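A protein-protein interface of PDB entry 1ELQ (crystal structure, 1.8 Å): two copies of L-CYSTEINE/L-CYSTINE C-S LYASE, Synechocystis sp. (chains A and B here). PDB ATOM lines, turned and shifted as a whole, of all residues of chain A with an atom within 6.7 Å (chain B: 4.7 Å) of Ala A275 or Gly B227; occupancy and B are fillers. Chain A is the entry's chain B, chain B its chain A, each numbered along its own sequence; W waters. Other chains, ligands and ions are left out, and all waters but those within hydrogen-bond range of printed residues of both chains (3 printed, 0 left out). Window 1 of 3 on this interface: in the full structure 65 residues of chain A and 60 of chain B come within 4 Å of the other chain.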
ATOM      1  N   TYR A  40      17.374  35.908 -17.085  1.00  0.00           N
ATOM      2  CA  TYR A  40      15.933  35.629 -16.799  1.00  0.00           C
ATOM      3  C   TYR A  40      15.242  36.946 -16.453  1.00  0.00           C
ATOM      4  O   TYR A  40      14.113  37.183 -16.867  1.00  0.00           O
ATOM      5  CB  TYR A  40      15.748  34.673 -15.619  1.00  0.00           C
ATOM      6  CG  TYR A  40      15.898  33.244 -15.987  1.00  0.00           C
ATOM      7  CD1 TYR A  40      16.974  32.497 -15.514  1.00  0.00           C
ATOM      8  CD2 TYR A  40      15.013  32.645 -16.887  1.00  0.00           C
ATOM      9  CE1 TYR A  40      17.178  31.172 -15.937  1.00  0.00           C
ATOM     10  CE2 TYR A  40      15.199  31.342 -17.307  1.00  0.00           C
ATOM     11  CZ  TYR A  40      16.283  30.614 -16.833  1.00  0.00           C
ATOM     12  OH  TYR A  40      16.483  29.336 -17.252  1.00  0.00           O
ATOM     13  N   LEU A  60      22.993  38.084 -27.767  1.00  0.00           N
ATOM     14  CA  LEU A  60      23.702  37.221 -26.830  1.00  0.00           C
ATOM     15  C   LEU A  60      24.291  35.994 -27.546  1.00  0.00           C
ATOM     16  O   LEU A  60      25.411  35.579 -27.237  1.00  0.00           O
ATOM     17  CB  LEU A  60      22.772  36.733 -25.703  1.00  0.00           C
ATOM     18  CG  LEU A  60      23.258  35.512 -24.909  1.00  0.00           C
ATOM     19  CD1 LEU A  60      24.484  35.854 -24.073  1.00  0.00           C
ATOM     20  CD2 LEU A  60      22.112  35.004 -23.999  1.00  0.00           C
ATOM     21  N   ASP A  83      24.092  21.921 -27.314  1.00  0.00           N
ATOM     22  CA  ASP A  83      23.826  21.728 -25.889  1.00  0.00           C
ATOM     23  C   ASP A  83      24.923  20.965 -25.172  1.00  0.00           C
ATOM     24  O   ASP A  83      25.041  21.048 -23.953  1.00  0.00           O
ATOM     25  CB  ASP A  83      22.582  20.881 -25.653  1.00  0.00           C
ATOM     26  CG  ASP A  83      21.346  21.468 -26.238  1.00  0.00           C
ATOM     27  OD1 ASP A  83      21.251  22.711 -26.350  1.00  0.00           O
ATOM     28  OD2 ASP A  83      20.449  20.652 -26.571  1.00  0.00           O
ATOM     29  N   GLY A 227      24.354  22.042 -20.333  1.00  0.00           N
ATOM     30  CA  GLY A 227      23.403  22.389 -21.370  1.00  0.00           C
ATOM     31  C   GLY A 227      23.860  23.277 -22.497  1.00  0.00           C
ATOM     32  O   GLY A 227      23.061  23.611 -23.359  1.00  0.00           O
ATOM     33  N   VAL A 228      25.125  23.693 -22.503  1.00  0.00           N
ATOM     34  CA  VAL A 228      25.585  24.534 -23.587  1.00  0.00           C
ATOM     35  C   VAL A 228      26.981  24.064 -24.029  1.00  0.00           C
ATOM     36  O   VAL A 228      27.892  23.959 -23.210  1.00  0.00           O
ATOM     37  CB  VAL A 228      25.695  25.999 -23.145  1.00  0.00           C
ATOM     38  CG1 VAL A 228      26.008  26.864 -24.357  1.00  0.00           C
ATOM     39  CG2 VAL A 228      24.365  26.461 -22.514  1.00  0.00           C
ATOM     40  N   ARG A 249      15.978  28.104 -36.541  1.00  0.00           N
ATOM     41  CA  ARG A 249      17.296  28.765 -36.443  1.00  0.00           C
ATOM     42  C   ARG A 249      18.230  28.330 -37.583  1.00  0.00           C
ATOM     43  O   ARG A 249      19.308  28.930 -37.783  1.00  0.00           O
ATOM     44  CB  ARG A 249      17.965  28.391 -35.117  1.00  0.00           C
ATOM     45  CG  ARG A 249      17.403  29.195 -33.921  1.00  0.00           C
ATOM     46  CD  ARG A 249      17.856  28.644 -32.589  1.00  0.00           C
ATOM     47  NE  ARG A 249      19.275  28.907 -32.329  1.00  0.00           N
ATOM     48  CZ  ARG A 249      19.939  28.392 -31.298  1.00  0.00           C
ATOM     49  NH1 ARG A 249      19.300  27.600 -30.445  1.00  0.00           N
ATOM     50  NH2 ARG A 249      21.247  28.647 -31.133  1.00  0.00           N
ATOM     51  N   ALA A 272      16.334  25.206 -32.703  1.00  0.00           N
ATOM     52  CA  ALA A 272      15.207  26.053 -32.323  1.00  0.00           C
ATOM     53  C   ALA A 272      15.341  26.573 -30.897  1.00  0.00           C
ATOM     54  O   ALA A 272      16.438  26.812 -30.430  1.00  0.00           O
ATOM     55  CB  ALA A 272      13.878  25.280 -32.497  1.00  0.00           C
ATOM     56  N   THR A 273      14.228  26.728 -30.180  1.00  0.00           N
ATOM     57  CA  THR A 273      14.360  27.311 -28.844  1.00  0.00           C
ATOM     58  C   THR A 273      15.305  26.573 -27.892  1.00  0.00           C
ATOM     59  O   THR A 273      15.201  25.367 -27.714  1.00  0.00           O
ATOM     60  CB  THR A 273      12.984  27.503 -28.190  1.00  0.00           C
ATOM     61  OG1 THR A 273      12.185  28.350 -29.017  1.00  0.00           O
ATOM     62  CG2 THR A 273      13.149  28.179 -26.839  1.00  0.00           C
ATOM     63  N   SER A 274      16.244  27.318 -27.312  1.00  0.00           N
ATOM     64  CA  SER A 274      17.240  26.794 -26.382  1.00  0.00           C
ATOM     65  C   SER A 274      17.201  27.591 -25.078  1.00  0.00           C
ATOM     66  O   SER A 274      16.576  28.641 -25.016  1.00  0.00           O
ATOM     67  CB  SER A 274      18.642  26.938 -26.987  1.00  0.00           C
ATOM     68  OG  SER A 274      18.856  26.035 -28.057  1.00  0.00           O
ATOM     69  N   ALA A 275      17.896  27.119 -24.048  1.00  0.00           N
ATOM     70  CA  ALA A 275      17.910  27.835 -22.761  1.00  0.00           C
ATOM     71  C   ALA A 275      18.888  29.029 -22.794  1.00  0.00           C
ATOM     72  O   ALA A 275      19.983  28.986 -22.229  1.00  0.00           O
ATOM     73  CB  ALA A 275      18.288  26.866 -21.643  1.00  0.00           C
ATOM     74  N   TYR A 276      18.475  30.093 -23.467  1.00  0.00           N
ATOM     75  CA  TYR A 276      19.286  31.290 -23.623  1.00  0.00           C
ATOM     76  C   TYR A 276      20.041  31.823 -22.402  1.00  0.00           C
ATOM     77  O   TYR A 276      21.248  32.160 -22.506  1.00  0.00           O
ATOM     78  CB  TYR A 276      18.416  32.376 -24.250  1.00  0.00           C
ATOM     79  CG  TYR A 276      17.673  31.857 -25.474  1.00  0.00           C
ATOM     80  CD1 TYR A 276      16.314  32.051 -25.612  1.00  0.00           C
ATOM     81  CD2 TYR A 276      18.351  31.213 -26.517  1.00  0.00           C
ATOM     82  CE1 TYR A 276      15.628  31.624 -26.765  1.00  0.00           C
ATOM     83  CE2 TYR A 276      17.698  30.797 -27.651  1.00  0.00           C
ATOM     84  CZ  TYR A 276      16.322  31.003 -27.778  1.00  0.00           C
ATOM     85  OH  TYR A 276      15.650  30.598 -28.922  1.00  0.00           O
ATOM     86  N   PRO A 277      19.377  31.941 -21.243  1.00  0.00           N
ATOM     87  CA  PRO A 277      20.084  32.445 -20.059  1.00  0.00           C
ATOM     88  C   PRO A 277      21.353  31.619 -19.803  1.00  0.00           C
ATOM     89  O   PRO A 277      22.346  32.117 -19.266  1.00  0.00           O
ATOM     90  CB  PRO A 277      19.052  32.271 -18.940  1.00  0.00           C
ATOM     91  CG  PRO A 277      17.745  32.495 -19.690  1.00  0.00           C
ATOM     92  CD  PRO A 277      17.957  31.657 -20.934  1.00  0.00           C
ATOM     93  N   GLN A 278      21.299  30.351 -20.189  1.00  0.00           N
ATOM     94  CA  GLN A 278      22.426  29.442 -20.028  1.00  0.00           C
ATOM     95  C   GLN A 278      23.595  29.897 -20.889  1.00  0.00           C
ATOM     96  O   GLN A 278      24.778  29.679 -20.534  1.00  0.00           O
ATOM     97  CB  GLN A 278      22.050  28.068 -20.506  1.00  0.00           C
ATOM     98  CG  GLN A 278      22.461  27.007 -19.600  1.00  0.00           C
ATOM     99  CD  GLN A 278      21.439  26.847 -18.560  1.00  0.00           C
ATOM    100  OE1 GLN A 278      20.381  27.476 -18.654  1.00  0.00           O
ATOM    101  NE2 GLN A 278      21.717  26.026 -17.551  1.00  0.00           N
ATOM    102  N   TYR A 279      23.248  30.503 -22.023  1.00  0.00           N
ATOM    103  CA  TYR A 279      24.269  30.990 -22.953  1.00  0.00           C
ATOM    104  C   TYR A 279      25.050  32.102 -22.289  1.00  0.00           C
ATOM    105  O   TYR A 279      26.280  32.174 -22.430  1.00  0.00           O
ATOM    106  CB  TYR A 279      23.636  31.521 -24.250  1.00  0.00           C
ATOM    107  CG  TYR A 279      23.095  30.472 -25.210  1.00  0.00           C
ATOM    108  CD1 TYR A 279      22.692  30.840 -26.472  1.00  0.00           C
ATOM    109  CD2 TYR A 279      23.025  29.124 -24.874  1.00  0.00           C
ATOM    110  CE1 TYR A 279      22.245  29.909 -27.395  1.00  0.00           C
ATOM    111  CE2 TYR A 279      22.557  28.171 -25.784  1.00  0.00           C
ATOM    112  CZ  TYR A 279      22.172  28.582 -27.054  1.00  0.00           C
ATOM    113  OH  TYR A 279      21.704  27.717 -28.002  1.00  0.00           O
ATOM    114  N   ALA A 280      24.351  32.985 -21.579  1.00  0.00           N
ATOM    115  CA  ALA A 280      25.025  34.068 -20.863  1.00  0.00           C
ATOM    116  C   ALA A 280      25.924  33.463 -19.757  1.00  0.00           C
ATOM    117  O   ALA A 280      27.020  33.995 -19.448  1.00  0.00           O
ATOM    118  CB  ALA A 280      23.986  35.050 -20.250  1.00  0.00           C
ATOM    119  N   THR B  82      12.638  16.804 -24.632  1.00  0.00           N
ATOM    120  CA  THR B  82      13.488  17.476 -25.618  1.00  0.00           C
ATOM    121  C   THR B  82      13.730  18.915 -25.132  1.00  0.00           C
ATOM    122  O   THR B  82      13.476  19.252 -23.978  1.00  0.00           O
ATOM    123  CB  THR B  82      12.765  17.567 -26.983  1.00  0.00           C
ATOM    124  OG1 THR B  82      11.601  18.400 -26.842  1.00  0.00           O
ATOM    125  CG2 THR B  82      12.320  16.160 -27.454  1.00  0.00           C
ATOM    126  N   ASP B  83      14.205  19.767 -26.026  1.00  0.00           N
ATOM    127  CA  ASP B  83      14.419  21.164 -25.673  1.00  0.00           C
ATOM    128  C   ASP B  83      13.368  22.078 -26.261  1.00  0.00           C
ATOM    129  O   ASP B  83      13.289  23.219 -25.850  1.00  0.00           O
ATOM    130  CB  ASP B  83      15.761  21.690 -26.207  1.00  0.00           C
ATOM    131  CG  ASP B  83      16.941  21.024 -25.583  1.00  0.00           C
ATOM    132  OD1 ASP B  83      16.783  20.420 -24.501  1.00  0.00           O
ATOM    133  OD2 ASP B  83      18.042  21.120 -26.176  1.00  0.00           O
ATOM    134  N   PRO B 225      10.504  27.537 -18.731  1.00  0.00           N
ATOM    135  CA  PRO B 225      11.573  28.369 -19.314  1.00  0.00           C
ATOM    136  C   PRO B 225      11.906  27.913 -20.733  1.00  0.00           C
ATOM    137  O   PRO B 225      11.627  26.775 -21.096  1.00  0.00           O
ATOM    138  CB  PRO B 225      12.757  28.114 -18.365  1.00  0.00           C
ATOM    139  CG  PRO B 225      12.542  26.745 -17.905  1.00  0.00           C
ATOM    140  CD  PRO B 225      11.028  26.671 -17.671  1.00  0.00           C
ATOM    141  N   ALA B 226      12.495  28.799 -21.538  1.00  0.00           N
ATOM    142  CA  ALA B 226      12.939  28.408 -22.874  1.00  0.00           C
ATOM    143  C   ALA B 226      13.982  27.271 -22.730  1.00  0.00           C
ATOM    144  O   ALA B 226      14.850  27.310 -21.844  1.00  0.00           O
ATOM    145  CB  ALA B 226      13.578  29.607 -23.593  1.00  0.00           C
ATOM    146  N   GLY B 227      13.876  26.253 -23.586  1.00  0.00           N
ATOM    147  CA  GLY B 227      14.837  25.159 -23.548  1.00  0.00           C
ATOM    148  C   GLY B 227      14.363  23.792 -23.108  1.00  0.00           C
ATOM    149  O   GLY B 227      15.166  22.861 -23.021  1.00  0.00           O
ATOM    150  N   VAL B 228      13.076  23.631 -22.815  1.00  0.00           N
ATOM    151  CA  VAL B 228      12.610  22.300 -22.437  1.00  0.00           C
ATOM    152  C   VAL B 228      11.246  22.036 -23.088  1.00  0.00           C
ATOM    153  O   VAL B 228      10.390  22.891 -23.047  1.00  0.00           O
ATOM    154  CB  VAL B 228      12.460  22.122 -20.902  1.00  0.00           C
ATOM    155  CG1 VAL B 228      12.368  20.597 -20.585  1.00  0.00           C
ATOM    156  CG2 VAL B 228      13.653  22.745 -20.147  1.00  0.00           C
ATOM    157  N   GLY B 229      11.096  20.876 -23.723  1.00  0.00           N
ATOM    158  CA  GLY B 229       9.843  20.500 -24.371  1.00  0.00           C
ATOM    159  C   GLY B 229       9.736  18.979 -24.327  1.00  0.00           C
ATOM    160  O   GLY B 229      10.407  18.307 -23.532  1.00  0.00           O
ATOM    161  N   ALA B 275      20.008  21.111 -19.882  1.00  0.00           N
ATOM    162  CA  ALA B 275      19.777  22.185 -18.926  1.00  0.00           C
ATOM    163  C   ALA B 275      18.861  21.669 -17.798  1.00  0.00           C
ATOM    164  O   ALA B 275      17.684  22.018 -17.731  1.00  0.00           O
ATOM    165  CB  ALA B 275      19.116  23.383 -19.668  1.00  0.00           C
ATOM    166  N   GLN B 278      16.566  23.837 -15.750  1.00  0.00           N
ATOM    167  CA  GLN B 278      15.400  24.282 -16.502  1.00  0.00           C
ATOM    168  C   GLN B 278      14.305  23.191 -16.481  1.00  0.00           C
ATOM    169  O   GLN B 278      13.111  23.498 -16.591  1.00  0.00           O
ATOM    170  CB  GLN B 278      15.783  24.674 -17.948  1.00  0.00           C
ATOM    171  CG  GLN B 278      16.436  26.106 -18.097  1.00  0.00           C
ATOM    172  CD  GLN B 278      17.788  26.198 -17.417  1.00  0.00           C
ATOM    173  OE1 GLN B 278      18.481  25.193 -17.285  1.00  0.00           O
ATOM    174  NE2 GLN B 278      18.191  27.428 -16.996  1.00  0.00           N
HETATM  175  O   HOH W   1      18.953  23.572 -26.791  1.00  0.00           O
HETATM  176  O   HOH W   2      15.500  29.409 -20.249  1.00  0.00           O
HETATM  177  O   HOH W   3      19.241  19.668 -24.418  1.00  0.00           O
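Asp A83 touches its own counterpart, Asp B83. Gly A227 touches Ala B275, and with the chains exchanged Ala A275 touches Gly B227. Gln B278 touches its own counterpart, Gln A278.
OD2 of Asp B83 sits close to OD2 of Asp A83 (2.5 Å). The side-chain hydroxyl of Tyr A40 sits at hydrogen-bond distance from the side-chain amide nitrogen of Gln B278, at 2.6 Å. The backbone carbonyl oxygen of Thr A273 lies close to the backbone carbonyl oxygen of Asp B83 (3.4 Å). NE2 of Gln B278 lies within hydrogen-bond range of OE1 of Gln A278, at 2.7 Å.
Among the printed residues, merely in contact across the chains: Gly A227 with Ala B275 (3.9 Å), Thr A273 with Ala B226 (3.6 Å), Thr A273 with Gly B227 (3.8 Å), Ser A274 with Ala B226 (3.5 Å), Ser A274 with Gly B227 (3.7 Å), Ala A275 with Ala B226 (3.2 Å) and Ala A275 with Gly B227 (3.7 Å).
Water W1 lies within hydrogen-bond range of the side-chain carboxylate (OD1) of Asp A83 (2.5 Å), the side-chain carboxylate (OD2) of Asp B83 (2.7 Å) and the side-chain hydroxyl (OG) of Ser A274 (2.8 Å). Water W3 lies within hydrogen-bond range of the side-chain carboxylate (OD1) of Asp B83 and the side-chain carboxylate (OD2) of Asp A83. Water W2 bridges the backbone carbonyl oxygen (O) of Ala B226 (2.7 Å) and the side-chain hydroxyl (OH) of Tyr A40 (3.2 Å).
Of the 9 printed residues of chain B, 5 touch a printed residue of chain A.
The backbone carbonyl oxygen (O) of Asp A83 sits at hydrogen-bond distance from the backbone NH (N) of Val A228 (3.0 Å). The backbone carbonyl oxygen of Asp B83 lies within hydrogen-bond range of the backbone NH of Val B228 (3.1 Å). The backbone carbonyl oxygen (O) of Ala B275 sits close to the side-chain amide oxygen (OE1) of Gln B278, at 3.3 Å. NH1 of Arg A249 is in hydrogen-bond range of OG of Ser A274 (2.9 Å). OG of Ser A274 sits at hydrogen-bond distance from OH of Tyr A279 (3.3 Å). The backbone carbonyl oxygen (O) of Ala A272 lies within hydrogen-bond range of the side-chain hydroxyl (OG) of Ser A274 (3.5 Å).
Printed residues of chain B within 4 Å of Tyr A40: Gln B278. Printed residues of chain B within 4 Å of Gly A227: Ala B275. Of the printed residues of chain A, Ala B226 touches Thr A273 (3.6 Å), Ser A274 (3.5 Å) and Ala A275 (3.2 Å). Gly B227 touches just these residues of chain A: Thr A273 (3.8 Å), Ser A274 (3.7 Å) and Ala A275 (3.7 Å). The nearest printed residue of chain B that does not touch Ala A275 is Gln B278 (4.1 Å). The nearest residue of chain A that does not touch Gly B227 is Tyr A276 (6.0 Å).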
